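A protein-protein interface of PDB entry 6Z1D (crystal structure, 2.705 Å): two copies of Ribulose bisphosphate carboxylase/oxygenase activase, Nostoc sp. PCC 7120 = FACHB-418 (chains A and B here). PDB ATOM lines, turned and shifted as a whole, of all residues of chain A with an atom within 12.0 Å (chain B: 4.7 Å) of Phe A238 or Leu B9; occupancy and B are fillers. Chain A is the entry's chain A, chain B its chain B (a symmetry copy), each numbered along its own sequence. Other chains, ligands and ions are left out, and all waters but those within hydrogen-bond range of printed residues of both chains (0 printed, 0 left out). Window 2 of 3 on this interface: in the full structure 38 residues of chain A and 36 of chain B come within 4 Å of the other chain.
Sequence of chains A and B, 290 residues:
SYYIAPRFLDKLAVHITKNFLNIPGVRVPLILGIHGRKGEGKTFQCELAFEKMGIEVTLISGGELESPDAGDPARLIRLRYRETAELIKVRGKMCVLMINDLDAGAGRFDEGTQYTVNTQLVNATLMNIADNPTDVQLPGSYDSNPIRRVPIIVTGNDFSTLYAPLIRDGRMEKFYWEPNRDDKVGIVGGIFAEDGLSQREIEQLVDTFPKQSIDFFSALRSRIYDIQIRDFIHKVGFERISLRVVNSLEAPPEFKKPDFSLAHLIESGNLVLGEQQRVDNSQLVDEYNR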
ATOM      1  N   ASP A 226      22.394   3.768 -23.148  1.00  0.00           N
ATOM      2  CA  ASP A 226      23.354   4.535 -22.362  1.00  0.00           C
ATOM      3  C   ASP A 226      23.439   5.975 -22.859  1.00  0.00           C
ATOM      4  O   ASP A 226      23.732   6.908 -22.102  1.00  0.00           O
ATOM      5  CB  ASP A 226      24.736   3.888 -22.412  1.00  0.00           C
ATOM      6  CG  ASP A 226      24.889   2.704 -21.445  1.00  0.00           C
ATOM      7  OD1 ASP A 226      23.870   2.197 -20.907  1.00  0.00           O
ATOM      8  OD2 ASP A 226      26.052   2.271 -21.231  1.00  0.00           O
ATOM      9  N   ILE A 227      23.136   6.154 -24.137  1.00  0.00           N
ATOM     10  CA  ILE A 227      23.342   7.441 -24.794  1.00  0.00           C
ATOM     11  C   ILE A 227      22.192   8.355 -24.435  1.00  0.00           C
ATOM     12  O   ILE A 227      22.403   9.486 -24.010  1.00  0.00           O
ATOM     13  CB  ILE A 227      23.411   7.318 -26.345  1.00  0.00           C
ATOM     14  CG1 ILE A 227      24.549   6.386 -26.789  1.00  0.00           C
ATOM     15  CG2 ILE A 227      23.579   8.714 -27.000  1.00  0.00           C
ATOM     16  CD1 ILE A 227      24.370   4.834 -26.498  1.00  0.00           C
ATOM     17  N   GLN A 228      20.977   7.857 -24.640  1.00  0.00           N
ATOM     18  CA  GLN A 228      19.776   8.503 -24.125  1.00  0.00           C
ATOM     19  C   GLN A 228      19.953   8.877 -22.651  1.00  0.00           C
ATOM     20  O   GLN A 228      19.621   9.992 -22.237  1.00  0.00           O
ATOM     21  CB  GLN A 228      18.577   7.567 -24.298  1.00  0.00           C
ATOM     22  CG  GLN A 228      18.140   7.402 -25.746  1.00  0.00           C
ATOM     23  CD  GLN A 228      16.793   6.712 -25.888  1.00  0.00           C
ATOM     24  OE1 GLN A 228      15.748   7.296 -25.605  1.00  0.00           O
ATOM     25  NE2 GLN A 228      16.816   5.464 -26.333  1.00  0.00           N
ATOM     26  N   ILE A 229      20.500   7.947 -21.873  1.00  0.00           N
ATOM     27  CA  ILE A 229      20.694   8.164 -20.446  1.00  0.00           C
ATOM     28  C   ILE A 229      21.676   9.311 -20.193  1.00  0.00           C
ATOM     29  O   ILE A 229      21.415  10.197 -19.368  1.00  0.00           O
ATOM     30  CB  ILE A 229      21.169   6.886 -19.725  1.00  0.00           C
ATOM     31  CG1 ILE A 229      20.056   5.837 -19.741  1.00  0.00           C
ATOM     32  CG2 ILE A 229      21.524   7.189 -18.271  1.00  0.00           C
ATOM     33  CD1 ILE A 229      20.539   4.432 -19.514  1.00  0.00           C
ATOM     34  N   ARG A 230      22.815   9.280 -20.883  1.00  0.00           N
ATOM     35  CA  ARG A 230      23.815  10.338 -20.725  1.00  0.00           C
ATOM     36  C   ARG A 230      23.223  11.685 -21.086  1.00  0.00           C
ATOM     37  O   ARG A 230      23.426  12.675 -20.382  1.00  0.00           O
ATOM     38  CB  ARG A 230      25.074  10.088 -21.574  1.00  0.00           C
ATOM     39  CG  ARG A 230      25.319  11.103 -22.710  1.00  0.00           C
ATOM     40  CD  ARG A 230      26.774  11.276 -23.130  1.00  0.00           C
ATOM     41  NE  ARG A 230      27.171  10.435 -24.266  1.00  0.00           N
ATOM     42  CZ  ARG A 230      26.689  10.566 -25.501  1.00  0.00           C
ATOM     43  NH1 ARG A 230      27.110   9.761 -26.475  1.00  0.00           N
ATOM     44  NH2 ARG A 230      25.773  11.494 -25.758  1.00  0.00           N
ATOM     45  N   ASP A 231      22.518  11.719 -22.208  1.00  0.00           N
ATOM     46  CA  ASP A 231      21.945  12.955 -22.711  1.00  0.00           C
ATOM     47  C   ASP A 231      20.916  13.460 -21.712  1.00  0.00           C
ATOM     48  O   ASP A 231      20.845  14.654 -21.433  1.00  0.00           O
ATOM     49  CB  ASP A 231      21.315  12.746 -24.100  1.00  0.00           C
ATOM     50  CG  ASP A 231      22.357  12.593 -25.219  1.00  0.00           C
ATOM     51  OD1 ASP A 231      23.556  12.897 -25.010  1.00  0.00           O
ATOM     52  OD2 ASP A 231      21.959  12.179 -26.329  1.00  0.00           O
ATOM     53  N   PHE A 232      20.128  12.532 -21.178  1.00  0.00           N
ATOM     54  CA  PHE A 232      19.159  12.845 -20.130  1.00  0.00           C
ATOM     55  C   PHE A 232      19.845  13.494 -18.921  1.00  0.00           C
ATOM     56  O   PHE A 232      19.307  14.428 -18.324  1.00  0.00           O
ATOM     57  CB  PHE A 232      18.399  11.579 -19.715  1.00  0.00           C
ATOM     58  CG  PHE A 232      17.538  11.753 -18.490  1.00  0.00           C
ATOM     59  CD1 PHE A 232      16.439  12.598 -18.509  1.00  0.00           C
ATOM     60  CD2 PHE A 232      17.820  11.055 -17.322  1.00  0.00           C
ATOM     61  CE1 PHE A 232      15.644  12.755 -17.381  1.00  0.00           C
ATOM     62  CE2 PHE A 232      17.028  11.206 -16.195  1.00  0.00           C
ATOM     63  CZ  PHE A 232      15.939  12.057 -16.226  1.00  0.00           C
ATOM     64  N   ILE A 233      21.038  13.009 -18.580  1.00  0.00           N
ATOM     65  CA  ILE A 233      21.814  13.570 -17.471  1.00  0.00           C
ATOM     66  C   ILE A 233      22.269  14.994 -17.783  1.00  0.00           C
ATOM     67  O   ILE A 233      22.190  15.882 -16.928  1.00  0.00           O
ATOM     68  CB  ILE A 233      23.046  12.691 -17.138  1.00  0.00           C
ATOM     69  CG1 ILE A 233      22.589  11.343 -16.575  1.00  0.00           C
ATOM     70  CG2 ILE A 233      23.951  13.381 -16.127  1.00  0.00           C
ATOM     71  CD1 ILE A 233      23.616  10.252 -16.652  1.00  0.00           C
ATOM     72  N   HIS A 234      22.742  15.204 -19.010  1.00  0.00           N
ATOM     73  CA  HIS A 234      23.181  16.526 -19.452  1.00  0.00           C
ATOM     74  C   HIS A 234      22.046  17.550 -19.424  1.00  0.00           C
ATOM     75  O   HIS A 234      22.260  18.708 -19.074  1.00  0.00           O
ATOM     76  CB  HIS A 234      23.770  16.452 -20.862  1.00  0.00           C
ATOM     77  CG  HIS A 234      25.043  15.669 -20.948  1.00  0.00           C
ATOM     78  ND1 HIS A 234      25.385  14.920 -22.056  1.00  0.00           N
ATOM     79  CD2 HIS A 234      26.052  15.510 -20.060  1.00  0.00           C
ATOM     80  CE1 HIS A 234      26.548  14.331 -21.844  1.00  0.00           C
ATOM     81  NE2 HIS A 234      26.977  14.677 -20.643  1.00  0.00           N
ATOM     82  N   LYS A 235      20.842  17.124 -19.797  1.00  0.00           N
ATOM     83  CA  LYS A 235      19.700  18.028 -19.832  1.00  0.00           C
ATOM     84  C   LYS A 235      19.331  18.492 -18.423  1.00  0.00           C
ATOM     85  O   LYS A 235      19.164  19.692 -18.172  1.00  0.00           O
ATOM     86  CB  LYS A 235      18.494  17.345 -20.479  1.00  0.00           C
ATOM     87  CG  LYS A 235      17.313  18.285 -20.691  1.00  0.00           C
ATOM     88  CD  LYS A 235      16.062  17.550 -21.148  1.00  0.00           C
ATOM     89  CE  LYS A 235      14.898  18.519 -21.295  1.00  0.00           C
ATOM     90  NZ  LYS A 235      13.798  17.975 -22.145  1.00  0.00           N
ATOM     91  N   VAL A 236      19.202  17.529 -17.514  1.00  0.00           N
ATOM     92  CA  VAL A 236      18.872  17.803 -16.116  1.00  0.00           C
ATOM     93  C   VAL A 236      20.026  18.505 -15.396  1.00  0.00           C
ATOM     94  O   VAL A 236      19.808  19.312 -14.486  1.00  0.00           O
ATOM     95  CB  VAL A 236      18.518  16.494 -15.375  1.00  0.00           C
ATOM     96  CG1 VAL A 236      18.325  16.734 -13.878  1.00  0.00           C
ATOM     97  CG2 VAL A 236      17.268  15.871 -15.974  1.00  0.00           C
ATOM     98  N   GLY A 237      21.251  18.192 -15.810  1.00  0.00           N
ATOM     99  CA  GLY A 237      22.438  18.789 -15.224  1.00  0.00           C
ATOM    100  C   GLY A 237      22.939  17.960 -14.063  1.00  0.00           C
ATOM    101  O   GLY A 237      22.148  17.460 -13.261  1.00  0.00           O
ATOM    102  N   PHE A 238      24.255  17.815 -13.972  1.00  0.00           N
ATOM    103  CA  PHE A 238      24.862  16.985 -12.941  1.00  0.00           C
ATOM    104  C   PHE A 238      24.510  17.457 -11.522  1.00  0.00           C
ATOM    105  O   PHE A 238      24.403  16.647 -10.605  1.00  0.00           O
ATOM    106  CB  PHE A 238      26.384  16.935 -13.126  1.00  0.00           C
ATOM    107  CG  PHE A 238      26.821  16.241 -14.390  1.00  0.00           C
ATOM    108  CD1 PHE A 238      26.840  14.861 -14.470  1.00  0.00           C
ATOM    109  CD2 PHE A 238      27.215  16.972 -15.495  1.00  0.00           C
ATOM    110  CE1 PHE A 238      27.237  14.225 -15.631  1.00  0.00           C
ATOM    111  CE2 PHE A 238      27.611  16.343 -16.655  1.00  0.00           C
ATOM    112  CZ  PHE A 238      27.623  14.967 -16.724  1.00  0.00           C
ATOM    113  N   GLU A 239      24.312  18.755 -11.336  1.00  0.00           N
ATOM    114  CA  GLU A 239      24.036  19.270 -10.000  1.00  0.00           C
ATOM    115  C   GLU A 239      22.724  18.728  -9.429  1.00  0.00           C
ATOM    116  O   GLU A 239      22.564  18.661  -8.209  1.00  0.00           O
ATOM    117  CB  GLU A 239      24.007  20.802 -10.003  1.00  0.00           C
ATOM    118  N   ARG A 240      21.801  18.334 -10.310  1.00  0.00           N
ATOM    119  CA  ARG A 240      20.430  17.997  -9.899  1.00  0.00           C
ATOM    120  C   ARG A 240      19.964  16.621 -10.365  1.00  0.00           C
ATOM    121  O   ARG A 240      18.778  16.305 -10.280  1.00  0.00           O
ATOM    122  CB  ARG A 240      19.446  19.059 -10.414  1.00  0.00           C
ATOM    123  N   ILE A 241      20.887  15.799 -10.850  1.00  0.00           N
ATOM    124  CA  ILE A 241      20.514  14.487 -11.363  1.00  0.00           C
ATOM    125  C   ILE A 241      20.039  13.567 -10.243  1.00  0.00           C
ATOM    126  O   ILE A 241      19.112  12.779 -10.434  1.00  0.00           O
ATOM    127  CB  ILE A 241      21.679  13.820 -12.133  1.00  0.00           C
ATOM    128  CG1 ILE A 241      21.267  12.447 -12.677  1.00  0.00           C
ATOM    129  CG2 ILE A 241      22.899  13.674 -11.248  1.00  0.00           C
ATOM    130  CD1 ILE A 241      20.072  12.472 -13.614  1.00  0.00           C
ATOM    131  N   SER A 242      20.667  13.674  -9.076  1.00  0.00           N
ATOM    132  CA  SER A 242      20.342  12.800  -7.952  1.00  0.00           C
ATOM    133  C   SER A 242      18.899  13.012  -7.499  1.00  0.00           C
ATOM    134  O   SER A 242      18.124  12.061  -7.408  1.00  0.00           O
ATOM    135  CB  SER A 242      21.302  13.050  -6.786  1.00  0.00           C
ATOM    136  OG  SER A 242      21.066  12.149  -5.715  1.00  0.00           O
ATOM    137  N   LEU A 243      18.556  14.265  -7.213  1.00  0.00           N
ATOM    138  CA  LEU A 243      17.201  14.639  -6.819  1.00  0.00           C
ATOM    139  C   LEU A 243      16.193  14.087  -7.822  1.00  0.00           C
ATOM    140  O   LEU A 243      15.189  13.493  -7.443  1.00  0.00           O
ATOM    141  CB  LEU A 243      17.093  16.174  -6.718  1.00  0.00           C
ATOM    142  CG  LEU A 243      15.759  16.859  -6.362  1.00  0.00           C
ATOM    143  CD1 LEU A 243      15.551  16.840  -4.869  1.00  0.00           C
ATOM    144  CD2 LEU A 243      15.749  18.331  -6.800  1.00  0.00           C
ATOM    145  N   ARG A 244      16.492  14.256  -9.104  1.00  0.00           N
ATOM    146  CA  ARG A 244      15.557  13.925 -10.178  1.00  0.00           C
ATOM    147  C   ARG A 244      15.176  12.445 -10.263  1.00  0.00           C
ATOM    148  O   ARG A 244      14.008  12.113 -10.477  1.00  0.00           O
ATOM    149  CB  ARG A 244      16.144  14.373 -11.519  1.00  0.00           C
ATOM    150  CG  ARG A 244      15.319  13.983 -12.748  1.00  0.00           C
ATOM    151  CD  ARG A 244      13.960  14.681 -12.802  1.00  0.00           C
ATOM    152  NE  ARG A 244      13.207  14.300 -14.002  1.00  0.00           N
ATOM    153  CZ  ARG A 244      12.230  13.393 -14.044  1.00  0.00           C
ATOM    154  NH1 ARG A 244      11.841  12.754 -12.946  1.00  0.00           N
ATOM    155  NH2 ARG A 244      11.627  13.128 -15.198  1.00  0.00           N
ATOM    156  N   VAL A 245      16.158  11.559 -10.124  1.00  0.00           N
ATOM    157  CA  VAL A 245      15.924  10.135 -10.350  1.00  0.00           C
ATOM    158  C   VAL A 245      15.357   9.435  -9.112  1.00  0.00           C
ATOM    159  O   VAL A 245      14.562   8.499  -9.239  1.00  0.00           O
ATOM    160  CB  VAL A 245      17.219   9.420 -10.788  1.00  0.00           C
ATOM    161  CG1 VAL A 245      16.953   7.937 -11.080  1.00  0.00           C
ATOM    162  CG2 VAL A 245      17.841  10.130 -12.000  1.00  0.00           C
ATOM    163  N   VAL A 246      15.747   9.895  -7.923  1.00  0.00           N
ATOM    164  CA  VAL A 246      15.435   9.174  -6.686  1.00  0.00           C
ATOM    165  C   VAL A 246      14.224   9.730  -5.950  1.00  0.00           C
ATOM    166  O   VAL A 246      13.431   8.973  -5.385  1.00  0.00           O
ATOM    167  CB  VAL A 246      16.633   9.142  -5.721  1.00  0.00           C
ATOM    168  CG1 VAL A 246      16.396   8.100  -4.635  1.00  0.00           C
ATOM    169  CG2 VAL A 246      17.919   8.840  -6.478  1.00  0.00           C
ATOM    170  N   ASN A 247      14.088  11.047  -5.916  1.00  0.00           N
ATOM    171  CA  ASN A 247      12.845  11.624  -5.454  1.00  0.00           C
ATOM    172  C   ASN A 247      11.769  11.442  -6.514  1.00  0.00           C
ATOM    173  O   ASN A 247      11.928  11.829  -7.676  1.00  0.00           O
ATOM    174  CB  ASN A 247      13.052  13.080  -5.071  1.00  0.00           C
ATOM    175  CG  ASN A 247      14.025  13.234  -3.925  1.00  0.00           C
ATOM    176  OD1 ASN A 247      15.154  13.723  -4.081  1.00  0.00           O
ATOM    177  ND2 ASN A 247      13.609  12.748  -2.768  1.00  0.00           N
ATOM    178  N   ILE B   4      37.545  17.587 -14.281  1.00  0.00           N
ATOM    179  CA  ILE B   4      37.079  16.218 -14.509  1.00  0.00           C
ATOM    180  C   ILE B   4      36.925  16.010 -16.018  1.00  0.00           C
ATOM    181  O   ILE B   4      36.281  16.811 -16.698  1.00  0.00           O
ATOM    182  CB  ILE B   4      35.749  15.936 -13.743  1.00  0.00           C
ATOM    183  CG1 ILE B   4      35.199  14.546 -14.059  1.00  0.00           C
ATOM    184  CG2 ILE B   4      34.675  16.964 -14.074  1.00  0.00           C
ATOM    185  CD1 ILE B   4      36.004  13.436 -13.504  1.00  0.00           C
ATOM    186  N   ALA B   5      37.539  14.960 -16.554  1.00  0.00           N
ATOM    187  CA  ALA B   5      37.477  14.712 -17.992  1.00  0.00           C
ATOM    188  C   ALA B   5      36.047  14.334 -18.377  1.00  0.00           C
ATOM    189  O   ALA B   5      35.495  13.383 -17.827  1.00  0.00           O
ATOM    190  CB  ALA B   5      38.451  13.619 -18.397  1.00  0.00           C
ATOM    191  N   PRO B   6      35.432  15.087 -19.311  1.00  0.00           N
ATOM    192  CA  PRO B   6      34.032  14.878 -19.701  1.00  0.00           C
ATOM    193  C   PRO B   6      33.596  13.422 -19.888  1.00  0.00           C
ATOM    194  O   PRO B   6      32.529  13.054 -19.398  1.00  0.00           O
ATOM    195  CB  PRO B   6      33.943  15.620 -21.025  1.00  0.00           C
ATOM    196  CG  PRO B   6      34.858  16.764 -20.839  1.00  0.00           C
ATOM    197  CD  PRO B   6      35.996  16.270 -19.990  1.00  0.00           C
ATOM    198  N   ARG B   7      34.390  12.612 -20.576  1.00  0.00           N
ATOM    199  CA  ARG B   7      33.981  11.239 -20.863  1.00  0.00           C
ATOM    200  C   ARG B   7      34.144  10.344 -19.640  1.00  0.00           C
ATOM    201  O   ARG B   7      33.506   9.295 -19.547  1.00  0.00           O
ATOM    202  CB  ARG B   7      34.748  10.669 -22.059  1.00  0.00           C
ATOM    203  CG  ARG B   7      36.190  10.358 -21.779  1.00  0.00           C
ATOM    204  CD  ARG B   7      36.951  10.054 -23.048  1.00  0.00           C
ATOM    205  NE  ARG B   7      38.386  10.154 -22.807  1.00  0.00           N
ATOM    206  CZ  ARG B   7      39.166   9.143 -22.434  1.00  0.00           C
ATOM    207  NH1 ARG B   7      40.453   9.360 -22.226  1.00  0.00           N
ATOM    208  NH2 ARG B   7      38.674   7.921 -22.276  1.00  0.00           N
ATOM    209  N   PHE B   8      34.997  10.763 -18.704  1.00  0.00           N
ATOM    210  CA  PHE B   8      35.118  10.082 -17.421  1.00  0.00           C
ATOM    211  C   PHE B   8      33.866  10.371 -16.611  1.00  0.00           C
ATOM    212  O   PHE B   8      33.254   9.461 -16.057  1.00  0.00           O
ATOM    213  CB  PHE B   8      36.355  10.559 -16.661  1.00  0.00           C
ATOM    214  CG  PHE B   8      36.766   9.644 -15.538  1.00  0.00           C
ATOM    215  CD1 PHE B   8      36.027   9.579 -14.368  1.00  0.00           C
ATOM    216  CD2 PHE B   8      37.894   8.854 -15.649  1.00  0.00           C
ATOM    217  CE1 PHE B   8      36.399   8.740 -13.338  1.00  0.00           C
ATOM    218  CE2 PHE B   8      38.272   8.017 -14.618  1.00  0.00           C
ATOM    219  CZ  PHE B   8      37.524   7.960 -13.461  1.00  0.00           C
ATOM    220  N   LEU B   9      33.490  11.646 -16.556  1.00  0.00           N
ATOM    221  CA  LEU B   9      32.291  12.080 -15.848  1.00  0.00           C
ATOM    222  C   LEU B   9      31.046  11.430 -16.436  1.00  0.00           C
ATOM    223  O   LEU B   9      30.154  11.019 -15.703  1.00  0.00           O
ATOM    224  CB  LEU B   9      32.155  13.609 -15.903  1.00  0.00           C
ATOM    225  CG  LEU B   9      30.902  14.228 -15.263  1.00  0.00           C
ATOM    226  CD1 LEU B   9      30.732  13.763 -13.813  1.00  0.00           C
ATOM    227  CD2 LEU B   9      30.941  15.746 -15.331  1.00  0.00           C
ATOM    228  N   ASP B  10      30.981  11.337 -17.759  1.00  0.00           N
ATOM    229  CA  ASP B  10      29.841  10.698 -18.408  1.00  0.00           C
ATOM    230  C   ASP B  10      29.743   9.230 -17.999  1.00  0.00           C
ATOM    231  O   ASP B  10      28.702   8.778 -17.519  1.00  0.00           O
ATOM    232  CB  ASP B  10      29.947  10.782 -19.932  1.00  0.00           C
ATOM    233  CG  ASP B  10      29.515  12.131 -20.494  1.00  0.00           C
ATOM    234  OD1 ASP B  10      29.000  12.978 -19.730  1.00  0.00           O
ATOM    235  OD2 ASP B  10      29.676  12.329 -21.721  1.00  0.00           O
ATOM    236  N   LYS B  11      30.831   8.489 -18.186  1.00  0.00           N
ATOM    237  CA  LYS B  11      30.808   7.046 -17.989  1.00  0.00           C
ATOM    238  C   LYS B  11      30.298   6.703 -16.601  1.00  0.00           C
ATOM    239  O   LYS B  11      29.426   5.855 -16.428  1.00  0.00           O
ATOM    240  CB  LYS B  11      32.210   6.470 -18.166  1.00  0.00           C
ATOM    241  CG  LYS B  11      32.249   4.955 -18.236  1.00  0.00           C
ATOM    242  CD  LYS B  11      31.575   4.454 -19.504  1.00  0.00           C
ATOM    243  CE  LYS B  11      31.671   2.948 -19.645  1.00  0.00           C
ATOM    244  NZ  LYS B  11      30.667   2.448 -20.610  1.00  0.00           N
ATOM    245  N   LEU B  12      30.851   7.400 -15.619  1.00  0.00           N
ATOM    246  CA  LEU B  12      30.538   7.165 -14.232  1.00  0.00           C
ATOM    247  C   LEU B  12      29.108   7.592 -13.915  1.00  0.00           C
ATOM    248  O   LEU B  12      28.367   6.856 -13.258  1.00  0.00           O
ATOM    249  CB  LEU B  12      31.532   7.936 -13.372  1.00  0.00           C
ATOM    250  CG  LEU B  12      31.446   7.755 -11.864  1.00  0.00           C
ATOM    251  CD1 LEU B  12      31.613   6.300 -11.475  1.00  0.00           C
ATOM    252  CD2 LEU B  12      32.508   8.604 -11.213  1.00  0.00           C
ATOM    253  N   ALA B  13      28.721   8.778 -14.384  1.00  0.00           N
ATOM    254  CA  ALA B  13      27.371   9.286 -14.152  1.00  0.00           C
ATOM    255  C   ALA B  13      26.315   8.385 -14.790  1.00  0.00           C
ATOM    256  O   ALA B  13      25.254   8.158 -14.205  1.00  0.00           O
ATOM    257  CB  ALA B  13      27.240  10.691 -14.678  1.00  0.00           C
ATOM    258  N   ALA B  49      33.630  13.722  -9.499  1.00  0.00           N
ATOM    259  CA  ALA B  49      32.296  13.458 -10.029  1.00  0.00           C
ATOM    260  C   ALA B  49      31.226  13.377  -8.929  1.00  0.00           C
ATOM    261  O   ALA B  49      30.133  13.914  -9.084  1.00  0.00           O
ATOM    262  CB  ALA B  49      32.312  12.184 -10.842  1.00  0.00           C
ATOM    263  N   LYS B  52      30.360  16.660  -7.419  1.00  0.00           N
ATOM    264  CA  LYS B  52      29.616  17.410  -8.421  1.00  0.00           C
ATOM    265  C   LYS B  52      28.153  16.995  -8.475  1.00  0.00           C
ATOM    266  O   LYS B  52      27.264  17.839  -8.609  1.00  0.00           O
ATOM    267  CB  LYS B  52      30.266  17.204  -9.791  1.00  0.00           C
ATOM    268  CG  LYS B  52      29.591  17.964 -10.904  1.00  0.00           C
ATOM    269  CD  LYS B  52      30.524  18.931 -11.586  1.00  0.00           C
ATOM    270  CE  LYS B  52      30.041  19.236 -12.983  1.00  0.00           C
ATOM    271  NZ  LYS B  52      30.773  20.373 -13.582  1.00  0.00           N
ATOM    272  N   MET B  53      27.908  15.694  -8.368  1.00  0.00           N
ATOM    273  CA  MET B  53      26.557  15.151  -8.441  1.00  0.00           C
ATOM    274  C   MET B  53      25.906  15.054  -7.074  1.00  0.00           C
ATOM    275  O   MET B  53      24.785  14.558  -6.943  1.00  0.00           O
ATOM    276  CB  MET B  53      26.595  13.767  -9.074  1.00  0.00           C
ATOM    277  CG  MET B  53      26.962  13.785 -10.535  1.00  0.00           C
ATOM    278  SD  MET B  53      26.813  12.149 -11.242  1.00  0.00           S
ATOM    279  CE  MET B  53      28.362  11.430 -10.723  1.00  0.00           C
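NE2 of His A234 lies within hydrogen-bond range of OD1 of Asp B10 (2.8 Å).
The side-chain carboxylate of Asp A231 is in salt-bridge range of the guanidinium group of Arg A230 (2.7 Å).
O of Arg A230 lies within hydrogen-bond range of ND1 of His A234, 3.4 Å away.
OD2 of Asp B10 touches CD of Arg A230, at 3.4 Å.
Ile A233 touches Ala B13.
Phe A238 touches Leu B9 (CE2 to CD2, 3.6 Å).
Asp B10 touches Phe A238.
Phe A238 touches Ala B13.
Phe A238 touches Lys B52 (O to O, 3.7 Å).
O of Phe A238 touches CA of Met B53, at 3.4 Å.
Lys B52 touches Glu A239 (O to CA, 3.8 Å).
CB of Ser A242 touches O of Met B53, 3.8 Å away.
Phe A238 touches just these residues of chain B: Leu B9, Asp B10, Ala B13, Lys B52 and Met B53.
Of chain A, only Phe A238 (3.6 Å) comes within 4 Å of Leu B9.
No residue of chain A comes within 4 Å of Ile B4.
No residue of chain A comes within 4 Å of Pro B6.
Phe B8 touches none of the printed residues of chain A.
Of the printed residues of chain A, Asp B10 touches Arg A230 (3.4 Å), His A234 (2.8 Å) and Phe A238 (3.9 Å).
Ala B13 touches just these residues of chain A: Ile A233 (3.6 Å) and Phe A238 (3.7 Å).
No residue of chain A comes within 4 Å of Ala B49.
Of chain A, only Phe A238 (3.4 Å) and Ser A242 (3.8 Å) come within 4 Å of Met B53.
Printed residues of chain B within 4 Å of Ser A242: Met B53.
Of the printed residues of chain B, Glu A239 touches Lys B52 (3.8 Å).
The nearest printed residue of chain B that does not touch Glu A239 is Met B53 (4.8 Å).
Printed residues of chain B that touch a printed residue of chain A: Leu B9, Asp B10, Ala B13, Lys B52 and Met B53.
Printed residues of chain A that touch a printed residue of chain B: Arg A230, Ile A233, His A234, Phe A238, Glu A239 and Ser A242.
Hydrophobic or aromatic side chains of chain A within 4 Å of the printed part of chain B: Ile A233, His A234 and Phe A238.
No position is printed for both chains.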
